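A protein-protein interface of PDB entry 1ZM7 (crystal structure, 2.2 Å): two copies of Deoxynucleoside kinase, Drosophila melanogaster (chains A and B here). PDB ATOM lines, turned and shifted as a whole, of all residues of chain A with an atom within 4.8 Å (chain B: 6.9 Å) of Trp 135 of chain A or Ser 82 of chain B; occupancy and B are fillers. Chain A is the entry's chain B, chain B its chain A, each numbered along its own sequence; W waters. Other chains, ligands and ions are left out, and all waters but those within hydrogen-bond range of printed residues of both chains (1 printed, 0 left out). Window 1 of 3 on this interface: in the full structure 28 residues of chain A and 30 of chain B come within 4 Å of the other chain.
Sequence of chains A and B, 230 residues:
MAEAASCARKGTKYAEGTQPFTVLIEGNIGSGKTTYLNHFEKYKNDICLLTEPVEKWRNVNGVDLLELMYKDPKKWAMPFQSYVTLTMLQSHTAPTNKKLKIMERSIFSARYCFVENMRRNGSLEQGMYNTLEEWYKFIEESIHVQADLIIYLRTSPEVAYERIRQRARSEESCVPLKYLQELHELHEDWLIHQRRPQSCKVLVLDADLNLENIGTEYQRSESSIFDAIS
The side-chain hydroxyl of Thr 87 of chain B sits close to the backbone carbonyl oxygen of Tyr 83 of chain B (3.5 Å). OE1 of Glu 134 of chain A lies within salt-bridge range of NZ of Lys 137 of chain A, at 3.4 Å. OG1 of Thr 85 of chain B lies within hydrogen-bond range of OH of Tyr 136 of chain B (2.8 Å). O of Gln 81 of chain B lies within hydrogen-bond range of OG1 of Thr 85 of chain B, 2.9 Å away.
Among the printed residues, pairs that only touch across the chains: Met 78 of chain A with Ser 82 of chain B (3.8 Å), Ser 82 of chain A with Met 78 of chain B (3.8 Å), Thr 131 of chain A with Leu 65 of chain B (3.7 Å), Thr 131 of chain A with Pro 79 of chain B (3.6 Å), Thr 131 of chain A with Ser 82 of chain B (3.8 Å), Thr 131 of chain A with Tyr 83 of chain B (3.7 Å), Glu 134 of chain A with Leu 86 of chain B (3.4 Å), Trp 135 of chain A with Thr 85 of chain B (3.9 Å), Trp 135 of chain A with Leu 86 of chain B (3.6 Å), Trp 135 of chain A with Leu 89 of chain B (3.6 Å), Trp 135 of chain A with Trp 135 of chain B (3.7 Å), Trp 135 of chain A with Ile 139 of chain B (3.96 Å), Phe 138 of chain A with Leu 86 of chain B (3.5 Å) and Phe 138 of chain A with Gln 90 of chain B (3.9 Å).
Water W1 lies within hydrogen-bond range of the backbone carbonyl oxygen of Glu 134 of chain A (2.7 Å) and the side-chain amide nitrogen of Gln 90 of chain B (2.8 Å).
Met 78 of chain A touches Ser 82 of chain B, and with the chains exchanged Ser 82 of chain A touches Met 78 of chain B. Ser 82 of chain A touches Trp 135 of chain B, and with the chains exchanged Trp 135 of chain A touches Ser 82 of chain B. Trp 135 of chain A touches its own counterpart, Trp 135 of chain B. Trp 135 of chain A touches Ile 139 of chain B, but with the chains exchanged Ile 139 of chain A does not touch Trp 135 of chain B (4.02 Å).
Hydrophobic or aromatic side chains of chain A that line the printed part of chain B: Met 78, Trp 135 and Phe 138. Of the 22 printed residues of chain B, 11 touch a printed residue of chain A. Hydrophobic or aromatic side chains of chain B within 4 Å of the printed part of chain A: Leu 65, Met 78, Pro 79, Tyr 83, Leu 86, Leu 89, Trp 135 and Ile 139. Along chain B the printed residues that touch a printed residue of chain A span positions 65 to 139. Among the printed residues, no Asp or Glu carboxylate lies within 4 Å of a Lys or Arg side-chain nitrogen of the other chain.
Printed residues of chain B within 4 Å of Ser 82 of chain A: Met 78 and Trp 135. Of the printed residues of chain A, Pro 79 of chain B touches Met 78 and Thr 131. Ser 82 of chain B touches just these residues of chain A: Met 78 (3.8 Å), Thr 131 (3.8 Å) and Trp 135 (3.0 Å). Of the printed residues of chain A, Tyr 83 of chain B touches Thr 131 (3.7 Å). Of the printed residues of chain A, Ile 139 of chain B touches Trp 135 (3.96 Å). The nearest printed residue of chain B that does not touch Met 78 of chain A is Phe 80 of chain B (5.6 Å).
SD of Met 78 of chain A sits close to N of Pro 79 of chain B (3.5 Å). OG of Ser 82 of chain A is in hydrogen-bond range of NE1 of Trp 135 of chain B. The indole nitrogen of Trp 135 of chain A is in hydrogen-bond range of the side-chain hydroxyl of Ser 82 of chain B (3.0 Å). The side-chain sulfur (SD) of Met 78 of chain A sits close to the side-chain sulfur (SD) of Met 78 of chain B.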
ATOM      1  N   MET A  78      11.085  22.135 -39.750  1.00  0.00           N
ATOM      2  CA  MET A  78      10.830  22.960 -38.529  1.00  0.00           C
ATOM      3  C   MET A  78      12.114  23.378 -37.797  1.00  0.00           C
ATOM      4  O   MET A  78      12.305  24.568 -37.571  1.00  0.00           O
ATOM      5  CB  MET A  78       9.890  22.223 -37.593  1.00  0.00           C
ATOM      6  CG  MET A  78       9.168  23.120 -36.599  1.00  0.00           C
ATOM      7  SD  MET A  78       9.739  22.857 -34.914  1.00  0.00           S
ATOM      8  CE  MET A  78       9.612  24.515 -34.253  1.00  0.00           C
ATOM      9  N   SER A  82      13.491  27.166 -37.654  1.00  0.00           N
ATOM     10  CA  SER A  82      13.744  27.704 -36.326  1.00  0.00           C
ATOM     11  C   SER A  82      15.176  28.272 -36.240  1.00  0.00           C
ATOM     12  O   SER A  82      15.398  29.353 -35.672  1.00  0.00           O
ATOM     13  CB  SER A  82      13.491  26.621 -35.279  1.00  0.00           C
ATOM     14  OG  SER A  82      13.809  27.121 -34.018  1.00  0.00           O
ATOM     15  N   THR A 131       3.607  26.606 -34.094  1.00  0.00           N
ATOM     16  CA  THR A 131       4.730  26.882 -33.179  1.00  0.00           C
ATOM     17  C   THR A 131       5.621  28.013 -33.716  1.00  0.00           C
ATOM     18  O   THR A 131       5.916  28.960 -32.994  1.00  0.00           O
ATOM     19  CB  THR A 131       5.536  25.588 -32.943  1.00  0.00           C
ATOM     20  OG1 THR A 131       4.668  24.624 -32.330  1.00  0.00           O
ATOM     21  CG2 THR A 131       6.642  25.814 -31.890  1.00  0.00           C
ATOM     22  N   LEU A 132       6.017  27.930 -34.981  1.00  0.00           N
ATOM     23  CA  LEU A 132       6.810  29.007 -35.598  1.00  0.00           C
ATOM     24  C   LEU A 132       6.068  30.344 -35.549  1.00  0.00           C
ATOM     25  O   LEU A 132       6.663  31.366 -35.178  1.00  0.00           O
ATOM     26  CB  LEU A 132       7.230  28.647 -37.036  1.00  0.00           C
ATOM     27  CG  LEU A 132       8.143  27.422 -37.188  1.00  0.00           C
ATOM     28  CD1 LEU A 132       8.194  26.905 -38.635  1.00  0.00           C
ATOM     29  CD2 LEU A 132       9.583  27.706 -36.670  1.00  0.00           C
ATOM     30  N   GLU A 133       4.772  30.341 -35.880  1.00  0.00           N
ATOM     31  CA  GLU A 133       3.984  31.592 -35.887  1.00  0.00           C
ATOM     32  C   GLU A 133       3.870  32.197 -34.496  1.00  0.00           C
ATOM     33  O   GLU A 133       3.980  33.416 -34.333  1.00  0.00           O
ATOM     34  CB  GLU A 133       2.580  31.377 -36.475  1.00  0.00           C
ATOM     35  CG  GLU A 133       2.580  31.336 -37.993  1.00  0.00           C
ATOM     36  CD  GLU A 133       2.874  32.705 -38.595  1.00  0.00           C
ATOM     37  OE1 GLU A 133       2.100  33.658 -38.370  1.00  0.00           O
ATOM     38  OE2 GLU A 133       3.902  32.848 -39.264  1.00  0.00           O
ATOM     39  N   GLU A 134       3.664  31.349 -33.496  1.00  0.00           N
ATOM     40  CA  GLU A 134       3.613  31.831 -32.118  1.00  0.00           C
ATOM     41  C   GLU A 134       4.955  32.436 -31.694  1.00  0.00           C
ATOM     42  O   GLU A 134       4.985  33.437 -30.975  1.00  0.00           O
ATOM     43  CB  GLU A 134       3.168  30.710 -31.163  1.00  0.00           C
ATOM     44  CG  GLU A 134       1.689  30.348 -31.239  1.00  0.00           C
ATOM     45  CD  GLU A 134       0.762  31.552 -31.191  1.00  0.00           C
ATOM     46  OE1 GLU A 134      -0.101  31.673 -32.096  1.00  0.00           O
ATOM     47  OE2 GLU A 134       0.896  32.393 -30.254  1.00  0.00           O
ATOM     48  N   TRP A 135       6.063  31.850 -32.157  1.00  0.00           N
ATOM     49  CA  TRP A 135       7.388  32.438 -31.921  1.00  0.00           C
ATOM     50  C   TRP A 135       7.510  33.804 -32.608  1.00  0.00           C
ATOM     51  O   TRP A 135       7.997  34.758 -31.992  1.00  0.00           O
ATOM     52  CB  TRP A 135       8.526  31.536 -32.429  1.00  0.00           C
ATOM     53  CG  TRP A 135       9.099  30.668 -31.342  1.00  0.00           C
ATOM     54  CD1 TRP A 135       8.879  29.327 -31.155  1.00  0.00           C
ATOM     55  CD2 TRP A 135       9.960  31.091 -30.277  1.00  0.00           C
ATOM     56  NE1 TRP A 135       9.563  28.890 -30.044  1.00  0.00           N
ATOM     57  CE2 TRP A 135      10.236  29.951 -29.484  1.00  0.00           C
ATOM     58  CE3 TRP A 135      10.518  32.336 -29.900  1.00  0.00           C
ATOM     59  CZ2 TRP A 135      11.070  30.000 -28.345  1.00  0.00           C
ATOM     60  CZ3 TRP A 135      11.355  32.389 -28.764  1.00  0.00           C
ATOM     61  CH2 TRP A 135      11.615  31.224 -28.004  1.00  0.00           C
ATOM     62  N   TYR A 136       7.087  33.892 -33.878  1.00  0.00           N
ATOM     63  CA  TYR A 136       7.134  35.182 -34.587  1.00  0.00           C
ATOM     64  C   TYR A 136       6.335  36.265 -33.861  1.00  0.00           C
ATOM     65  O   TYR A 136       6.799  37.397 -33.748  1.00  0.00           O
ATOM     66  CB  TYR A 136       6.708  35.074 -36.051  1.00  0.00           C
ATOM     67  CG  TYR A 136       7.694  34.317 -36.908  1.00  0.00           C
ATOM     68  CD1 TYR A 136       7.297  33.189 -37.627  1.00  0.00           C
ATOM     69  CD2 TYR A 136       9.025  34.719 -36.999  1.00  0.00           C
ATOM     70  CE1 TYR A 136       8.196  32.494 -38.402  1.00  0.00           C
ATOM     71  CE2 TYR A 136       9.924  34.034 -37.781  1.00  0.00           C
ATOM     72  CZ  TYR A 136       9.504  32.922 -38.473  1.00  0.00           C
ATOM     73  OH  TYR A 136      10.385  32.226 -39.242  1.00  0.00           O
ATOM     74  N   LYS A 137       5.168  35.903 -33.328  1.00  0.00           N
ATOM     75  CA  LYS A 137       4.339  36.869 -32.600  1.00  0.00           C
ATOM     76  C   LYS A 137       5.021  37.312 -31.313  1.00  0.00           C
ATOM     77  O   LYS A 137       4.995  38.491 -30.976  1.00  0.00           O
ATOM     78  CB  LYS A 137       2.953  36.306 -32.298  1.00  0.00           C
ATOM     79  CG  LYS A 137       2.122  36.084 -33.549  1.00  0.00           C
ATOM     80  CD  LYS A 137       0.814  35.361 -33.189  1.00  0.00           C
ATOM     81  CE  LYS A 137      -0.018  35.059 -34.427  1.00  0.00           C
ATOM     82  NZ  LYS A 137      -1.220  34.248 -34.034  1.00  0.00           N
ATOM     83  N   PHE A 138       5.639  36.376 -30.600  1.00  0.00           N
ATOM     84  CA  PHE A 138       6.422  36.755 -29.427  1.00  0.00           C
ATOM     85  C   PHE A 138       7.631  37.634 -29.774  1.00  0.00           C
ATOM     86  O   PHE A 138       7.973  38.540 -29.014  1.00  0.00           O
ATOM     87  CB  PHE A 138       6.902  35.536 -28.652  1.00  0.00           C
ATOM     88  CG  PHE A 138       7.707  35.887 -27.430  1.00  0.00           C
ATOM     89  CD1 PHE A 138       7.084  36.422 -26.298  1.00  0.00           C
ATOM     90  CD2 PHE A 138       9.086  35.728 -27.423  1.00  0.00           C
ATOM     91  CE1 PHE A 138       7.822  36.736 -25.170  1.00  0.00           C
ATOM     92  CE2 PHE A 138       9.831  36.069 -26.309  1.00  0.00           C
ATOM     93  CZ  PHE A 138       9.201  36.557 -25.173  1.00  0.00           C
ATOM     94  N   ILE A 139       8.287  37.344 -30.894  1.00  0.00           N
ATOM     95  CA  ILE A 139       9.439  38.136 -31.323  1.00  0.00           C
ATOM     96  C   ILE A 139       9.018  39.601 -31.638  1.00  0.00           C
ATOM     97  O   ILE A 139       9.707  40.554 -31.250  1.00  0.00           O
ATOM     98  CB  ILE A 139      10.160  37.447 -32.517  1.00  0.00           C
ATOM     99  CG1 ILE A 139      10.970  36.230 -32.026  1.00  0.00           C
ATOM    100  CG2 ILE A 139      11.062  38.414 -33.271  1.00  0.00           C
ATOM    101  CD1 ILE A 139      11.235  35.168 -33.097  1.00  0.00           C
ATOM    102  N   LEU B  65      -0.153  19.052 -29.191  1.00  0.00           N
ATOM    103  CA  LEU B  65       1.294  18.852 -29.411  1.00  0.00           C
ATOM    104  C   LEU B  65       1.868  17.809 -28.468  1.00  0.00           C
ATOM    105  O   LEU B  65       2.755  17.051 -28.859  1.00  0.00           O
ATOM    106  CB  LEU B  65       2.102  20.145 -29.247  1.00  0.00           C
ATOM    107  CG  LEU B  65       2.179  21.205 -30.348  1.00  0.00           C
ATOM    108  CD1 LEU B  65       3.124  22.317 -29.885  1.00  0.00           C
ATOM    109  CD2 LEU B  65       2.623  20.648 -31.705  1.00  0.00           C
ATOM    110  N   TRP B  76       8.288  15.069 -33.645  1.00  0.00           N
ATOM    111  CA  TRP B  76       7.537  16.074 -32.898  1.00  0.00           C
ATOM    112  C   TRP B  76       8.208  16.598 -31.629  1.00  0.00           C
ATOM    113  O   TRP B  76       7.769  17.604 -31.090  1.00  0.00           O
ATOM    114  CB  TRP B  76       6.101  15.596 -32.575  1.00  0.00           C
ATOM    115  CG  TRP B  76       5.222  15.640 -33.786  1.00  0.00           C
ATOM    116  CD1 TRP B  76       4.920  14.593 -34.625  1.00  0.00           C
ATOM    117  CD2 TRP B  76       4.555  16.788 -34.324  1.00  0.00           C
ATOM    118  NE1 TRP B  76       4.110  15.029 -35.648  1.00  0.00           N
ATOM    119  CE2 TRP B  76       3.870  16.368 -35.494  1.00  0.00           C
ATOM    120  CE3 TRP B  76       4.462  18.126 -33.944  1.00  0.00           C
ATOM    121  CZ2 TRP B  76       3.099  17.234 -36.263  1.00  0.00           C
ATOM    122  CZ3 TRP B  76       3.713  18.997 -34.722  1.00  0.00           C
ATOM    123  CH2 TRP B  76       3.023  18.541 -35.855  1.00  0.00           C
ATOM    124  N   ALA B  77       9.238  15.921 -31.143  1.00  0.00           N
ATOM    125  CA  ALA B  77       9.927  16.389 -29.941  1.00  0.00           C
ATOM    126  C   ALA B  77      10.507  17.798 -30.122  1.00  0.00           C
ATOM    127  O   ALA B  77      10.399  18.622 -29.217  1.00  0.00           O
ATOM    128  CB  ALA B  77      11.006  15.402 -29.482  1.00  0.00           C
ATOM    129  N   MET B  78      11.100  18.097 -31.284  1.00  0.00           N
ATOM    130  CA  MET B  78      11.685  19.462 -31.480  1.00  0.00           C
ATOM    131  C   MET B  78      10.637  20.579 -31.490  1.00  0.00           C
ATOM    132  O   MET B  78      10.745  21.513 -30.686  1.00  0.00           O
ATOM    133  CB  MET B  78      12.532  19.552 -32.747  1.00  0.00           C
ATOM    134  CG  MET B  78      13.539  20.688 -32.708  1.00  0.00           C
ATOM    135  SD  MET B  78      13.290  21.864 -34.049  1.00  0.00           S
ATOM    136  CE  MET B  78      13.967  23.357 -33.319  1.00  0.00           C
ATOM    137  N   PRO B  79       9.614  20.527 -32.349  1.00  0.00           N
ATOM    138  CA  PRO B  79       8.583  21.583 -32.301  1.00  0.00           C
ATOM    139  C   PRO B  79       7.879  21.623 -30.937  1.00  0.00           C
ATOM    140  O   PRO B  79       7.571  22.710 -30.428  1.00  0.00           O
ATOM    141  CB  PRO B  79       7.607  21.200 -33.425  1.00  0.00           C
ATOM    142  CG  PRO B  79       7.874  19.746 -33.711  1.00  0.00           C
ATOM    143  CD  PRO B  79       9.354  19.531 -33.410  1.00  0.00           C
ATOM    144  N   PHE B  80       7.646  20.470 -30.323  1.00  0.00           N
ATOM    145  CA  PHE B  80       7.041  20.473 -28.990  1.00  0.00           C
ATOM    146  C   PHE B  80       7.921  21.211 -27.947  1.00  0.00           C
ATOM    147  O   PHE B  80       7.431  22.062 -27.212  1.00  0.00           O
ATOM    148  CB  PHE B  80       6.730  19.048 -28.511  1.00  0.00           C
ATOM    149  CG  PHE B  80       6.238  19.000 -27.099  1.00  0.00           C
ATOM    150  CD1 PHE B  80       4.925  19.278 -26.805  1.00  0.00           C
ATOM    151  CD2 PHE B  80       7.110  18.706 -26.060  1.00  0.00           C
ATOM    152  CE1 PHE B  80       4.480  19.268 -25.468  1.00  0.00           C
ATOM    153  CE2 PHE B  80       6.674  18.670 -24.751  1.00  0.00           C
ATOM    154  CZ  PHE B  80       5.356  18.957 -24.455  1.00  0.00           C
ATOM    155  N   GLN B  81       9.215  20.890 -27.882  1.00  0.00           N
ATOM    156  CA  GLN B  81      10.096  21.574 -26.926  1.00  0.00           C
ATOM    157  C   GLN B  81      10.252  23.043 -27.273  1.00  0.00           C
ATOM    158  O   GLN B  81      10.378  23.903 -26.392  1.00  0.00           O
ATOM    159  CB  GLN B  81      11.490  20.920 -26.840  1.00  0.00           C
ATOM    160  CG  GLN B  81      11.499  19.596 -26.095  1.00  0.00           C
ATOM    161  CD  GLN B  81      10.899  19.657 -24.688  1.00  0.00           C
ATOM    162  OE1 GLN B  81      10.208  18.732 -24.296  1.00  0.00           O
ATOM    163  NE2 GLN B  81      11.189  20.735 -23.911  1.00  0.00           N
ATOM    164  N   SER B  82      10.220  23.332 -28.559  1.00  0.00           N
ATOM    165  CA  SER B  82      10.258  24.723 -28.984  1.00  0.00           C
ATOM    166  C   SER B  82       9.024  25.477 -28.462  1.00  0.00           C
ATOM    167  O   SER B  82       9.127  26.618 -27.965  1.00  0.00           O
ATOM    168  CB  SER B  82      10.378  24.788 -30.507  1.00  0.00           C
ATOM    169  OG  SER B  82      10.325  26.129 -30.911  1.00  0.00           O
ATOM    170  N   TYR B  83       7.855  24.854 -28.545  1.00  0.00           N
ATOM    171  CA  TYR B  83       6.643  25.479 -28.051  1.00  0.00           C
ATOM    172  C   TYR B  83       6.664  25.588 -26.519  1.00  0.00           C
ATOM    173  O   TYR B  83       6.271  26.609 -25.958  1.00  0.00           O
ATOM    174  CB  TYR B  83       5.372  24.753 -28.535  1.00  0.00           C
ATOM    175  CG  TYR B  83       4.110  25.528 -28.225  1.00  0.00           C
ATOM    176  CD1 TYR B  83       3.838  26.741 -28.860  1.00  0.00           C
ATOM    177  CD2 TYR B  83       3.217  25.075 -27.263  1.00  0.00           C
ATOM    178  CE1 TYR B  83       2.674  27.485 -28.554  1.00  0.00           C
ATOM    179  CE2 TYR B  83       2.055  25.793 -26.954  1.00  0.00           C
ATOM    180  CZ  TYR B  83       1.795  26.993 -27.607  1.00  0.00           C
ATOM    181  OH  TYR B  83       0.665  27.684 -27.285  1.00  0.00           O
ATOM    182  N   VAL B  84       7.134  24.549 -25.842  1.00  0.00           N
ATOM    183  CA  VAL B  84       7.309  24.633 -24.382  1.00  0.00           C
ATOM    184  C   VAL B  84       8.164  25.847 -24.006  1.00  0.00           C
ATOM    185  O   VAL B  84       7.806  26.630 -23.114  1.00  0.00           O
ATOM    186  CB  VAL B  84       7.947  23.333 -23.771  1.00  0.00           C
ATOM    187  CG1 VAL B  84       8.351  23.561 -22.305  1.00  0.00           C
ATOM    188  CG2 VAL B  84       6.979  22.163 -23.864  1.00  0.00           C
ATOM    189  N   THR B  85       9.280  26.015 -24.699  1.00  0.00           N
ATOM    190  CA  THR B  85      10.199  27.121 -24.428  1.00  0.00           C
ATOM    191  C   THR B  85       9.478  28.442 -24.572  1.00  0.00           C
ATOM    192  O   THR B  85       9.575  29.325 -23.711  1.00  0.00           O
ATOM    193  CB  THR B  85      11.389  27.062 -25.400  1.00  0.00           C
ATOM    194  OG1 THR B  85      12.131  25.871 -25.150  1.00  0.00           O
ATOM    195  CG2 THR B  85      12.388  28.228 -25.143  1.00  0.00           C
ATOM    196  N   LEU B  86       8.733  28.576 -25.652  1.00  0.00           N
ATOM    197  CA  LEU B  86       7.999  29.793 -25.902  1.00  0.00           C
ATOM    198  C   LEU B  86       6.995  30.099 -24.789  1.00  0.00           C
ATOM    199  O   LEU B  86       6.952  31.236 -24.298  1.00  0.00           O
ATOM    200  CB  LEU B  86       7.287  29.752 -27.255  1.00  0.00           C
ATOM    201  CG  LEU B  86       6.353  30.949 -27.501  1.00  0.00           C
ATOM    202  CD1 LEU B  86       7.201  32.227 -27.616  1.00  0.00           C
ATOM    203  CD2 LEU B  86       5.560  30.716 -28.779  1.00  0.00           C
ATOM    204  N   THR B  87       6.186  29.111 -24.400  1.00  0.00           N
ATOM    205  CA  THR B  87       5.165  29.381 -23.385  1.00  0.00           C
ATOM    206  C   THR B  87       5.798  29.758 -22.055  1.00  0.00           C
ATOM    207  O   THR B  87       5.271  30.593 -21.358  1.00  0.00           O
ATOM    208  CB  THR B  87       4.149  28.215 -23.203  1.00  0.00           C
ATOM    209  OG1 THR B  87       4.841  27.021 -22.839  1.00  0.00           O
ATOM    210  CG2 THR B  87       3.468  27.856 -24.525  1.00  0.00           C
ATOM    211  N   LEU B  89       8.760  31.306 -21.616  1.00  0.00           N
ATOM    212  CA  LEU B  89       9.182  32.683 -21.857  1.00  0.00           C
ATOM    213  C   LEU B  89       8.035  33.690 -21.721  1.00  0.00           C
ATOM    214  O   LEU B  89       8.203  34.745 -21.114  1.00  0.00           O
ATOM    215  CB  LEU B  89       9.775  32.794 -23.242  1.00  0.00           C
ATOM    216  CG  LEU B  89      11.158  33.365 -23.432  1.00  0.00           C
ATOM    217  CD1 LEU B  89      12.038  33.209 -22.174  1.00  0.00           C
ATOM    218  CD2 LEU B  89      11.749  32.689 -24.669  1.00  0.00           C
ATOM    219  N   GLN B  90       6.874  33.369 -22.288  1.00  0.00           N
ATOM    220  CA  GLN B  90       5.707  34.243 -22.161  1.00  0.00           C
ATOM    221  C   GLN B  90       5.292  34.359 -20.690  1.00  0.00           C
ATOM    222  O   GLN B  90       4.883  35.434 -20.248  1.00  0.00           O
ATOM    223  CB  GLN B  90       4.534  33.765 -23.022  1.00  0.00           C
ATOM    224  CG  GLN B  90       4.840  33.777 -24.526  1.00  0.00           C
ATOM    225  CD  GLN B  90       3.745  33.143 -25.364  1.00  0.00           C
ATOM    226  OE1 GLN B  90       3.264  32.055 -25.052  1.00  0.00           O
ATOM    227  NE2 GLN B  90       3.355  33.822 -26.438  1.00  0.00           N
ATOM    228  N   ILE B 107      11.720  27.802 -17.959  1.00  0.00           N
ATOM    229  CA  ILE B 107      12.541  27.521 -19.118  1.00  0.00           C
ATOM    230  C   ILE B 107      13.733  26.601 -18.754  1.00  0.00           C
ATOM    231  O   ILE B 107      14.214  25.835 -19.601  1.00  0.00           O
ATOM    232  CB  ILE B 107      12.976  28.860 -19.774  1.00  0.00           C
ATOM    233  CG1 ILE B 107      13.559  28.607 -21.160  1.00  0.00           C
ATOM    234  CG2 ILE B 107      13.981  29.625 -18.871  1.00  0.00           C
ATOM    235  CD1 ILE B 107      13.721  29.873 -22.000  1.00  0.00           C
ATOM    236  N   VAL B 115      14.881  18.590 -22.578  1.00  0.00           N
ATOM    237  CA  VAL B 115      15.669  18.602 -23.810  1.00  0.00           C
ATOM    238  C   VAL B 115      16.883  17.645 -23.682  1.00  0.00           C
ATOM    239  O   VAL B 115      17.169  16.872 -24.594  1.00  0.00           O
ATOM    240  CB  VAL B 115      16.113  20.047 -24.214  1.00  0.00           C
ATOM    241  CG1 VAL B 115      17.131  19.991 -25.348  1.00  0.00           C
ATOM    242  CG2 VAL B 115      14.874  20.882 -24.630  1.00  0.00           C
ATOM    243  N   LEU B 132      17.930  24.009 -30.506  1.00  0.00           N
ATOM    244  CA  LEU B 132      17.345  24.386 -29.220  1.00  0.00           C
ATOM    245  C   LEU B 132      18.384  25.061 -28.314  1.00  0.00           C
ATOM    246  O   LEU B 132      18.104  26.107 -27.714  1.00  0.00           O
ATOM    247  CB  LEU B 132      16.686  23.185 -28.514  1.00  0.00           C
ATOM    248  CG  LEU B 132      15.494  22.541 -29.257  1.00  0.00           C
ATOM    249  CD1 LEU B 132      15.156  21.148 -28.718  1.00  0.00           C
ATOM    250  CD2 LEU B 132      14.234  23.454 -29.215  1.00  0.00           C
ATOM    251  N   TRP B 135      19.141  28.546 -29.371  1.00  0.00           N
ATOM    252  CA  TRP B 135      18.030  29.394 -28.931  1.00  0.00           C
ATOM    253  C   TRP B 135      18.164  29.738 -27.436  1.00  0.00           C
ATOM    254  O   TRP B 135      17.987  30.908 -27.056  1.00  0.00           O
ATOM    255  CB  TRP B 135      16.659  28.739 -29.160  1.00  0.00           C
ATOM    256  CG  TRP B 135      16.026  29.171 -30.456  1.00  0.00           C
ATOM    257  CD1 TRP B 135      15.941  28.441 -31.614  1.00  0.00           C
ATOM    258  CD2 TRP B 135      15.425  30.442 -30.731  1.00  0.00           C
ATOM    259  NE1 TRP B 135      15.305  29.180 -32.590  1.00  0.00           N
ATOM    260  CE2 TRP B 135      14.976  30.412 -32.076  1.00  0.00           C
ATOM    261  CE3 TRP B 135      15.218  31.611 -29.973  1.00  0.00           C
ATOM    262  CZ2 TRP B 135      14.316  31.498 -32.681  1.00  0.00           C
ATOM    263  CZ3 TRP B 135      14.553  32.699 -30.571  1.00  0.00           C
ATOM    264  CH2 TRP B 135      14.123  32.631 -31.916  1.00  0.00           C
ATOM    265  N   TYR B 136      18.431  28.729 -26.600  1.00  0.00           N
ATOM    266  CA  TYR B 136      18.611  28.989 -25.163  1.00  0.00           C
ATOM    267  C   TYR B 136      19.728  30.003 -24.897  1.00  0.00           C
ATOM    268  O   TYR B 136      19.560  30.889 -24.060  1.00  0.00           O
ATOM    269  CB  TYR B 136      18.833  27.708 -24.348  1.00  0.00           C
ATOM    270  CG  TYR B 136      17.596  26.840 -24.263  1.00  0.00           C
ATOM    271  CD1 TYR B 136      17.621  25.519 -24.697  1.00  0.00           C
ATOM    272  CD2 TYR B 136      16.400  27.340 -23.759  1.00  0.00           C
ATOM    273  CE1 TYR B 136      16.507  24.727 -24.626  1.00  0.00           C
ATOM    274  CE2 TYR B 136      15.270  26.550 -23.670  1.00  0.00           C
ATOM    275  CZ  TYR B 136      15.332  25.250 -24.112  1.00  0.00           C
ATOM    276  OH  TYR B 136      14.222  24.464 -24.041  1.00  0.00           O
ATOM    277  N   ILE B 139      18.449  33.375 -25.782  1.00  0.00           N
ATOM    278  CA  ILE B 139      17.473  33.813 -24.777  1.00  0.00           C
ATOM    279  C   ILE B 139      18.188  34.364 -23.513  1.00  0.00           C
ATOM    280  O   ILE B 139      17.800  35.398 -22.969  1.00  0.00           O
ATOM    281  CB  ILE B 139      16.474  32.661 -24.449  1.00  0.00           C
ATOM    282  CG1 ILE B 139      15.461  32.490 -25.601  1.00  0.00           C
ATOM    283  CG2 ILE B 139      15.748  32.899 -23.135  1.00  0.00           C
ATOM    284  CD1 ILE B 139      14.825  31.089 -25.686  1.00  0.00           C
ATOM    285  N   ILE B 143      16.633  38.040 -23.091  1.00  0.00           N
ATOM    286  CA  ILE B 143      15.375  38.041 -22.336  1.00  0.00           C
ATOM    287  C   ILE B 143      15.694  37.874 -20.864  1.00  0.00           C
ATOM    288  O   ILE B 143      16.467  36.986 -20.481  1.00  0.00           O
ATOM    289  CB  ILE B 143      14.402  36.906 -22.791  1.00  0.00           C
ATOM    290  CG1 ILE B 143      14.299  36.813 -24.330  1.00  0.00           C
ATOM    291  CG2 ILE B 143      13.044  37.055 -22.113  1.00  0.00           C
ATOM    292  CD1 ILE B 143      13.278  37.733 -24.981  1.00  0.00           C
HETATM  293  O   HOH W   1       3.013  34.019 -29.233  1.00  0.00           O
